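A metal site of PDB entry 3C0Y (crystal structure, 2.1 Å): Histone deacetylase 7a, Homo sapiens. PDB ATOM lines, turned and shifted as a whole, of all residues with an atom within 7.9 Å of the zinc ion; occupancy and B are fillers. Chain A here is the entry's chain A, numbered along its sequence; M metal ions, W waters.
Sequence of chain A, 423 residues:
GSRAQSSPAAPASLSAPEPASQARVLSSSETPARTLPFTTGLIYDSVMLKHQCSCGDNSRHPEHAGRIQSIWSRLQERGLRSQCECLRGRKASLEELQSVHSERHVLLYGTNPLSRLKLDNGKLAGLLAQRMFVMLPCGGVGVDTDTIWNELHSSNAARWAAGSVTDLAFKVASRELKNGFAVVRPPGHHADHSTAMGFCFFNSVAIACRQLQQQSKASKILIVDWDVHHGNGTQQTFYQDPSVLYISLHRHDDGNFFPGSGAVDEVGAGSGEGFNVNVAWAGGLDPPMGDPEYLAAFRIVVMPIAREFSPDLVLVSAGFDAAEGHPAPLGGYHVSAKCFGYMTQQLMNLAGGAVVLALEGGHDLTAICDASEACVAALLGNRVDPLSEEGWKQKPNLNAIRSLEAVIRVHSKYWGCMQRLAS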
ATOM      1  N   ARG A  67      -8.200 -34.440 -24.018  1.00  0.00           N
ATOM      2  CA  ARG A  67      -9.198 -33.595 -23.334  1.00  0.00           C
ATOM      3  C   ARG A  67     -10.462 -33.386 -24.147  1.00  0.00           C
ATOM      4  O   ARG A  67     -11.557 -33.629 -23.647  1.00  0.00           O
ATOM      5  CB  ARG A  67      -8.634 -32.241 -22.870  1.00  0.00           C
ATOM      6  CG  ARG A  67      -7.332 -32.337 -22.085  1.00  0.00           C
ATOM      7  CD  ARG A  67      -6.714 -30.990 -21.796  1.00  0.00           C
ATOM      8  NE  ARG A  67      -7.697 -30.111 -21.156  1.00  0.00           N
ATOM      9  CZ  ARG A  67      -8.164 -28.987 -21.688  1.00  0.00           C
ATOM     10  NH1 ARG A  67      -7.711 -28.559 -22.880  1.00  0.00           N
ATOM     11  NH2 ARG A  67      -9.079 -28.288 -21.043  1.00  0.00           N
ATOM     12  N   PRO A 187      -6.587 -23.789 -24.931  1.00  0.00           N
ATOM     13  CA  PRO A 187      -7.376 -22.841 -24.195  1.00  0.00           C
ATOM     14  C   PRO A 187      -6.920 -21.417 -24.498  1.00  0.00           C
ATOM     15  O   PRO A 187      -5.924 -21.250 -25.222  1.00  0.00           O
ATOM     16  CB  PRO A 187      -7.066 -23.216 -22.715  1.00  0.00           C
ATOM     17  CG  PRO A 187      -5.626 -23.703 -22.821  1.00  0.00           C
ATOM     18  CD  PRO A 187      -5.673 -24.530 -24.057  1.00  0.00           C
ATOM     19  N   HIS A 189      -7.489 -18.164 -22.070  1.00  0.00           N
ATOM     20  CA  HIS A 189      -7.702 -17.022 -21.194  1.00  0.00           C
ATOM     21  C   HIS A 189      -6.431 -16.462 -20.524  1.00  0.00           C
ATOM     22  O   HIS A 189      -6.439 -15.325 -20.034  1.00  0.00           O
ATOM     23  CB  HIS A 189      -8.855 -17.298 -20.205  1.00  0.00           C
ATOM     24  CG  HIS A 189      -8.480 -18.199 -19.092  1.00  0.00           C
ATOM     25  ND1 HIS A 189      -8.944 -18.013 -17.804  1.00  0.00           N
ATOM     26  CD2 HIS A 189      -7.709 -19.320 -19.059  1.00  0.00           C
ATOM     27  CE1 HIS A 189      -8.462 -18.967 -17.032  1.00  0.00           C
ATOM     28  NE2 HIS A 189      -7.712 -19.770 -17.760  1.00  0.00           N
ATOM     29  N   HIS A 190      -5.306 -17.165 -20.641  1.00  0.00           N
ATOM     30  CA  HIS A 190      -4.035 -16.621 -20.205  1.00  0.00           C
ATOM     31  C   HIS A 190      -3.284 -15.806 -21.301  1.00  0.00           C
ATOM     32  O   HIS A 190      -2.317 -15.158 -21.007  1.00  0.00           O
ATOM     33  CB  HIS A 190      -3.143 -17.784 -19.735  1.00  0.00           C
ATOM     34  CG  HIS A 190      -3.673 -18.505 -18.520  1.00  0.00           C
ATOM     35  ND1 HIS A 190      -3.929 -17.868 -17.334  1.00  0.00           N
ATOM     36  CD2 HIS A 190      -3.951 -19.826 -18.319  1.00  0.00           C
ATOM     37  CE1 HIS A 190      -4.396 -18.755 -16.441  1.00  0.00           C
ATOM     38  NE2 HIS A 190      -4.385 -19.961 -17.018  1.00  0.00           N
ATOM     39  N   GLY A 198       0.797 -20.325 -20.413  1.00  0.00           N
ATOM     40  CA  GLY A 198      -0.245 -21.059 -19.728  1.00  0.00           C
ATOM     41  C   GLY A 198      -1.083 -21.958 -20.625  1.00  0.00           C
ATOM     42  O   GLY A 198      -2.262 -22.185 -20.357  1.00  0.00           O
ATOM     43  N   PHE A 199      -0.464 -22.502 -21.667  1.00  0.00           N
ATOM     44  CA  PHE A 199      -1.144 -23.389 -22.606  1.00  0.00           C
ATOM     45  C   PHE A 199      -1.970 -22.710 -23.718  1.00  0.00           C
ATOM     46  O   PHE A 199      -2.507 -23.416 -24.588  1.00  0.00           O
ATOM     47  CB  PHE A 199      -1.953 -24.473 -21.885  1.00  0.00           C
ATOM     48  CG  PHE A 199      -1.165 -25.245 -20.862  1.00  0.00           C
ATOM     49  CD1 PHE A 199      -0.088 -26.001 -21.222  1.00  0.00           C
ATOM     50  CD2 PHE A 199      -1.506 -25.174 -19.512  1.00  0.00           C
ATOM     51  CE1 PHE A 199       0.654 -26.744 -20.235  1.00  0.00           C
ATOM     52  CE2 PHE A 199      -0.771 -25.883 -18.502  1.00  0.00           C
ATOM     53  CZ  PHE A 199       0.299 -26.655 -18.879  1.00  0.00           C
ATOM     54  N   CYS A 200      -1.950 -21.361 -23.700  1.00  0.00           N
ATOM     55  CA  CYS A 200      -2.836 -20.462 -24.466  1.00  0.00           C
ATOM     56  C   CYS A 200      -2.043 -19.618 -25.436  1.00  0.00           C
ATOM     57  O   CYS A 200      -0.948 -19.142 -25.108  1.00  0.00           O
ATOM     58  CB  CYS A 200      -3.547 -19.461 -23.523  1.00  0.00           C
ATOM     59  SG  CYS A 200      -4.568 -20.196 -22.224  1.00  0.00           S
ATOM     60  N   ASP A 225     -15.477 -16.084 -15.692  1.00  0.00           N
ATOM     61  CA  ASP A 225     -14.377 -16.994 -15.870  1.00  0.00           C
ATOM     62  C   ASP A 225     -14.347 -17.935 -14.623  1.00  0.00           C
ATOM     63  O   ASP A 225     -13.955 -17.484 -13.539  1.00  0.00           O
ATOM     64  CB  ASP A 225     -13.090 -16.173 -15.999  1.00  0.00           C
ATOM     65  CG  ASP A 225     -11.840 -17.015 -16.277  1.00  0.00           C
ATOM     66  OD1 ASP A 225     -11.740 -18.192 -15.906  1.00  0.00           O
ATOM     67  OD2 ASP A 225     -10.951 -16.519 -16.960  1.00  0.00           O
ATOM     68  N   TRP A 226     -14.787 -19.187 -14.760  1.00  0.00           N
ATOM     69  CA  TRP A 226     -14.741 -20.099 -13.594  1.00  0.00           C
ATOM     70  C   TRP A 226     -13.636 -21.152 -13.630  1.00  0.00           C
ATOM     71  O   TRP A 226     -13.576 -22.004 -12.776  1.00  0.00           O
ATOM     72  CB  TRP A 226     -16.116 -20.692 -13.251  1.00  0.00           C
ATOM     73  CG  TRP A 226     -16.701 -21.755 -14.269  1.00  0.00           C
ATOM     74  CD1 TRP A 226     -16.059 -22.815 -14.822  1.00  0.00           C
ATOM     75  CD2 TRP A 226     -18.037 -21.775 -14.789  1.00  0.00           C
ATOM     76  NE1 TRP A 226     -16.953 -23.537 -15.642  1.00  0.00           N
ATOM     77  CE2 TRP A 226     -18.157 -22.890 -15.630  1.00  0.00           C
ATOM     78  CE3 TRP A 226     -19.170 -20.960 -14.590  1.00  0.00           C
ATOM     79  CZ2 TRP A 226     -19.356 -23.212 -16.269  1.00  0.00           C
ATOM     80  CZ3 TRP A 226     -20.342 -21.286 -15.223  1.00  0.00           C
ATOM     81  CH2 TRP A 226     -20.426 -22.410 -16.038  1.00  0.00           C
ATOM     82  N   ASP A 227     -12.705 -21.070 -14.577  1.00  0.00           N
ATOM     83  CA  ASP A 227     -11.518 -21.842 -14.498  1.00  0.00           C
ATOM     84  C   ASP A 227     -10.834 -21.459 -13.134  1.00  0.00           C
ATOM     85  O   ASP A 227     -10.953 -20.289 -12.684  1.00  0.00           O
ATOM     86  CB  ASP A 227     -10.646 -21.432 -15.677  1.00  0.00           C
ATOM     87  CG  ASP A 227      -9.437 -22.271 -15.837  1.00  0.00           C
ATOM     88  OD1 ASP A 227      -8.474 -22.147 -15.033  1.00  0.00           O
ATOM     89  OD2 ASP A 227      -9.369 -23.025 -16.822  1.00  0.00           O
ATOM     90  N   VAL A 228     -10.124 -22.412 -12.528  1.00  0.00           N
ATOM     91  CA  VAL A 228      -9.552 -22.177 -11.187  1.00  0.00           C
ATOM     92  C   VAL A 228      -8.422 -21.150 -11.198  1.00  0.00           C
ATOM     93  O   VAL A 228      -8.046 -20.624 -10.158  1.00  0.00           O
ATOM     94  CB  VAL A 228      -9.091 -23.504 -10.505  1.00  0.00           C
ATOM     95  CG1 VAL A 228      -7.748 -23.967 -11.075  1.00  0.00           C
ATOM     96  CG2 VAL A 228      -8.999 -23.312  -8.981  1.00  0.00           C
ATOM     97  N   HIS A 229      -7.846 -20.901 -12.378  1.00  0.00           N
ATOM     98  CA  HIS A 229      -6.765 -19.918 -12.557  1.00  0.00           C
ATOM     99  C   HIS A 229      -7.349 -18.596 -13.023  1.00  0.00           C
ATOM    100  O   HIS A 229      -8.387 -18.576 -13.732  1.00  0.00           O
ATOM    101  CB  HIS A 229      -5.813 -20.375 -13.623  1.00  0.00           C
ATOM    102  CG  HIS A 229      -5.136 -21.664 -13.320  1.00  0.00           C
ATOM    103  ND1 HIS A 229      -5.472 -22.846 -13.964  1.00  0.00           N
ATOM    104  CD2 HIS A 229      -4.099 -21.943 -12.490  1.00  0.00           C
ATOM    105  CE1 HIS A 229      -4.698 -23.813 -13.490  1.00  0.00           C
ATOM    106  NE2 HIS A 229      -3.836 -23.282 -12.616  1.00  0.00           N
ATOM    107  N   HIS A 230      -6.732 -17.494 -12.604  1.00  0.00           N
ATOM    108  CA  HIS A 230      -7.094 -16.159 -13.071  1.00  0.00           C
ATOM    109  C   HIS A 230      -6.818 -16.042 -14.593  1.00  0.00           C
ATOM    110  O   HIS A 230      -5.763 -16.446 -15.079  1.00  0.00           O
ATOM    111  CB  HIS A 230      -6.297 -15.081 -12.299  1.00  0.00           C
ATOM    112  CG  HIS A 230      -6.580 -13.692 -12.722  1.00  0.00           C
ATOM    113  ND1 HIS A 230      -7.841 -13.128 -12.675  1.00  0.00           N
ATOM    114  CD2 HIS A 230      -5.760 -12.728 -13.185  1.00  0.00           C
ATOM    115  CE1 HIS A 230      -7.784 -11.883 -13.113  1.00  0.00           C
ATOM    116  NE2 HIS A 230      -6.530 -11.625 -13.429  1.00  0.00           N
ATOM    117  N   GLY A 231      -7.810 -15.528 -15.308  1.00  0.00           N
ATOM    118  CA  GLY A 231      -7.693 -15.246 -16.764  1.00  0.00           C
ATOM    119  C   GLY A 231      -7.045 -13.888 -16.953  1.00  0.00           C
ATOM    120  O   GLY A 231      -7.691 -12.882 -17.227  1.00  0.00           O
ATOM    121  N   PHE A 257      -0.439 -18.668  -6.542  1.00  0.00           N
ATOM    122  CA  PHE A 257      -1.014 -19.690  -7.451  1.00  0.00           C
ATOM    123  C   PHE A 257      -0.953 -19.183  -8.930  1.00  0.00           C
ATOM    124  O   PHE A 257      -1.121 -17.984  -9.180  1.00  0.00           O
ATOM    125  CB  PHE A 257      -2.425 -20.021  -7.003  1.00  0.00           C
ATOM    126  CG  PHE A 257      -2.985 -21.296  -7.626  1.00  0.00           C
ATOM    127  CD1 PHE A 257      -2.429 -22.553  -7.318  1.00  0.00           C
ATOM    128  CD2 PHE A 257      -4.070 -21.241  -8.522  1.00  0.00           C
ATOM    129  CE1 PHE A 257      -2.915 -23.707  -7.897  1.00  0.00           C
ATOM    130  CE2 PHE A 257      -4.563 -22.407  -9.081  1.00  0.00           C
ATOM    131  CZ  PHE A 257      -3.992 -23.626  -8.779  1.00  0.00           C
ATOM    132  N   PHE A 258      -0.640 -20.072  -9.886  1.00  0.00           N
ATOM    133  CA  PHE A 258      -0.526 -19.680 -11.289  1.00  0.00           C
ATOM    134  C   PHE A 258      -1.803 -18.916 -11.716  1.00  0.00           C
ATOM    135  O   PHE A 258      -2.888 -19.353 -11.419  1.00  0.00           O
ATOM    136  CB  PHE A 258      -0.298 -20.914 -12.193  1.00  0.00           C
ATOM    137  CG  PHE A 258      -0.018 -20.571 -13.619  1.00  0.00           C
ATOM    138  CD1 PHE A 258      -1.057 -20.537 -14.568  1.00  0.00           C
ATOM    139  CD2 PHE A 258       1.286 -20.206 -14.021  1.00  0.00           C
ATOM    140  CE1 PHE A 258      -0.803 -20.144 -15.910  1.00  0.00           C
ATOM    141  CE2 PHE A 258       1.536 -19.816 -15.347  1.00  0.00           C
ATOM    142  CZ  PHE A 258       0.477 -19.782 -16.307  1.00  0.00           C
ATOM    143  N   PRO A 259      -1.655 -17.763 -12.387  1.00  0.00           N
ATOM    144  CA  PRO A 259      -0.387 -17.087 -12.721  1.00  0.00           C
ATOM    145  C   PRO A 259       0.118 -15.976 -11.769  1.00  0.00           C
ATOM    146  O   PRO A 259       1.002 -15.222 -12.168  1.00  0.00           O
ATOM    147  CB  PRO A 259      -0.703 -16.448 -14.069  1.00  0.00           C
ATOM    148  CG  PRO A 259      -2.190 -16.049 -13.908  1.00  0.00           C
ATOM    149  CD  PRO A 259      -2.808 -17.158 -13.106  1.00  0.00           C
ATOM    150  N   GLY A 319     -13.424 -23.361 -17.607  1.00  0.00           N
ATOM    151  CA  GLY A 319     -12.393 -24.326 -17.358  1.00  0.00           C
ATOM    152  C   GLY A 319     -12.981 -25.228 -16.299  1.00  0.00           C
ATOM    153  O   GLY A 319     -13.855 -24.784 -15.550  1.00  0.00           O
ATOM    154  N   PHE A 320     -12.531 -26.476 -16.254  1.00  0.00           N
ATOM    155  CA  PHE A 320     -13.035 -27.411 -15.198  1.00  0.00           C
ATOM    156  C   PHE A 320     -11.980 -27.890 -14.222  1.00  0.00           C
ATOM    157  O   PHE A 320     -12.145 -28.937 -13.600  1.00  0.00           O
ATOM    158  CB  PHE A 320     -13.855 -28.570 -15.797  1.00  0.00           C
ATOM    159  CG  PHE A 320     -15.031 -28.086 -16.560  1.00  0.00           C
ATOM    160  CD1 PHE A 320     -15.091 -28.225 -17.931  1.00  0.00           C
ATOM    161  CD2 PHE A 320     -16.040 -27.375 -15.913  1.00  0.00           C
ATOM    162  CE1 PHE A 320     -16.167 -27.733 -18.642  1.00  0.00           C
ATOM    163  CE2 PHE A 320     -17.125 -26.875 -16.582  1.00  0.00           C
ATOM    164  CZ  PHE A 320     -17.203 -27.059 -17.967  1.00  0.00           C
ATOM    165  N   ASP A 321     -10.924 -27.098 -14.063  1.00  0.00           N
ATOM    166  CA  ASP A 321      -9.828 -27.453 -13.221  1.00  0.00           C
ATOM    167  C   ASP A 321     -10.035 -27.229 -11.713  1.00  0.00           C
ATOM    168  O   ASP A 321      -9.154 -27.530 -10.891  1.00  0.00           O
ATOM    169  CB  ASP A 321      -8.495 -26.878 -13.742  1.00  0.00           C
ATOM    170  CG  ASP A 321      -8.585 -25.420 -14.234  1.00  0.00           C
ATOM    171  OD1 ASP A 321      -9.649 -24.741 -14.168  1.00  0.00           O
ATOM    172  OD2 ASP A 321      -7.522 -24.990 -14.728  1.00  0.00           O
ATOM    173  N   ALA A 322     -11.207 -26.675 -11.390  1.00  0.00           N
ATOM    174  CA  ALA A 322     -11.664 -26.539 -10.032  1.00  0.00           C
ATOM    175  C   ALA A 322     -12.516 -27.768  -9.699  1.00  0.00           C
ATOM    176  O   ALA A 322     -13.012 -27.850  -8.604  1.00  0.00           O
ATOM    177  CB  ALA A 322     -12.501 -25.241  -9.857  1.00  0.00           C
ATOM    178  N   LEU A 330      -2.373 -28.455  -9.640  1.00  0.00           N
ATOM    179  CA  LEU A 330      -3.187 -27.869 -10.702  1.00  0.00           C
ATOM    180  C   LEU A 330      -4.644 -27.630 -10.262  1.00  0.00           C
ATOM    181  O   LEU A 330      -5.553 -27.610 -11.114  1.00  0.00           O
ATOM    182  CB  LEU A 330      -3.163 -28.756 -11.963  1.00  0.00           C
ATOM    183  CG  LEU A 330      -1.866 -29.435 -12.438  1.00  0.00           C
ATOM    184  CD1 LEU A 330      -1.776 -30.890 -11.884  1.00  0.00           C
ATOM    185  CD2 LEU A 330      -1.673 -29.389 -13.996  1.00  0.00           C
ATOM    186  N   GLU A 360     -11.889 -23.982 -21.372  1.00  0.00           N
ATOM    187  CA  GLU A 360     -10.579 -23.487 -20.979  1.00  0.00           C
ATOM    188  C   GLU A 360      -9.701 -24.610 -20.420  1.00  0.00           C
ATOM    189  O   GLU A 360      -9.265 -25.478 -21.193  1.00  0.00           O
ATOM    190  CB  GLU A 360     -10.680 -22.320 -20.001  1.00  0.00           C
ATOM    191  CG  GLU A 360     -11.441 -21.091 -20.557  1.00  0.00           C
ATOM    192  CD  GLU A 360     -10.667 -20.238 -21.627  1.00  0.00           C
ATOM    193  OE1 GLU A 360     -11.226 -19.233 -22.152  1.00  0.00           O
ATOM    194  OE2 GLU A 360      -9.490 -20.490 -21.910  1.00  0.00           O
ATOM    195  N   GLY A 361      -9.432 -24.591 -19.111  1.00  0.00           N
ATOM    196  CA  GLY A 361      -8.554 -25.625 -18.521  1.00  0.00           C
ATOM    197  C   GLY A 361      -9.310 -26.822 -17.914  1.00  0.00           C
ATOM    198  O   GLY A 361     -10.509 -26.951 -18.044  1.00  0.00           O
ATOM    199  N   GLY A 362      -8.614 -27.682 -17.219  1.00  0.00           N
ATOM    200  CA  GLY A 362      -9.255 -28.871 -16.659  1.00  0.00           C
ATOM    201  C   GLY A 362      -8.737 -29.987 -17.536  1.00  0.00           C
ATOM    202  O   GLY A 362      -8.954 -29.946 -18.746  1.00  0.00           O
HETATM  203 ZN    ZN M   1      -6.987 -23.174 -15.440  1.00  0.00          ZN
HETATM  204  O   HOH W   1      -5.988 -21.897 -17.160  1.00  0.00           O
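The side-chain carboxylate of Asp 321 is in hydrogen-bond range of the backbone NH of Val 228, at 2.9 Å. OD1 of Asp 225 sits at hydrogen-bond distance from N of Asp 227. The side-chain carboxylate (OD2) of Asp 227 lies within hydrogen-bond range of the backbone NH (N) of Gly 361, 2.8 Å away.
Three residues have an atom within 4 Å of the zinc ion: Asp 227, His 229 and Asp 321.
The zinc ion is bound by OD1 of Asp 227 (1.9 Å), OD2 of Asp 321 (2.0 Å), ND1 of His 229 (2.1 Å) and water W1 (2.4 Å). Slightly farther from the zinc ion lies OD2 of Asp 227 (2.8 Å).
Water W1 bridges NE2 of His 190 (2.5 Å) and NE2 of His 189 (2.8 Å).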
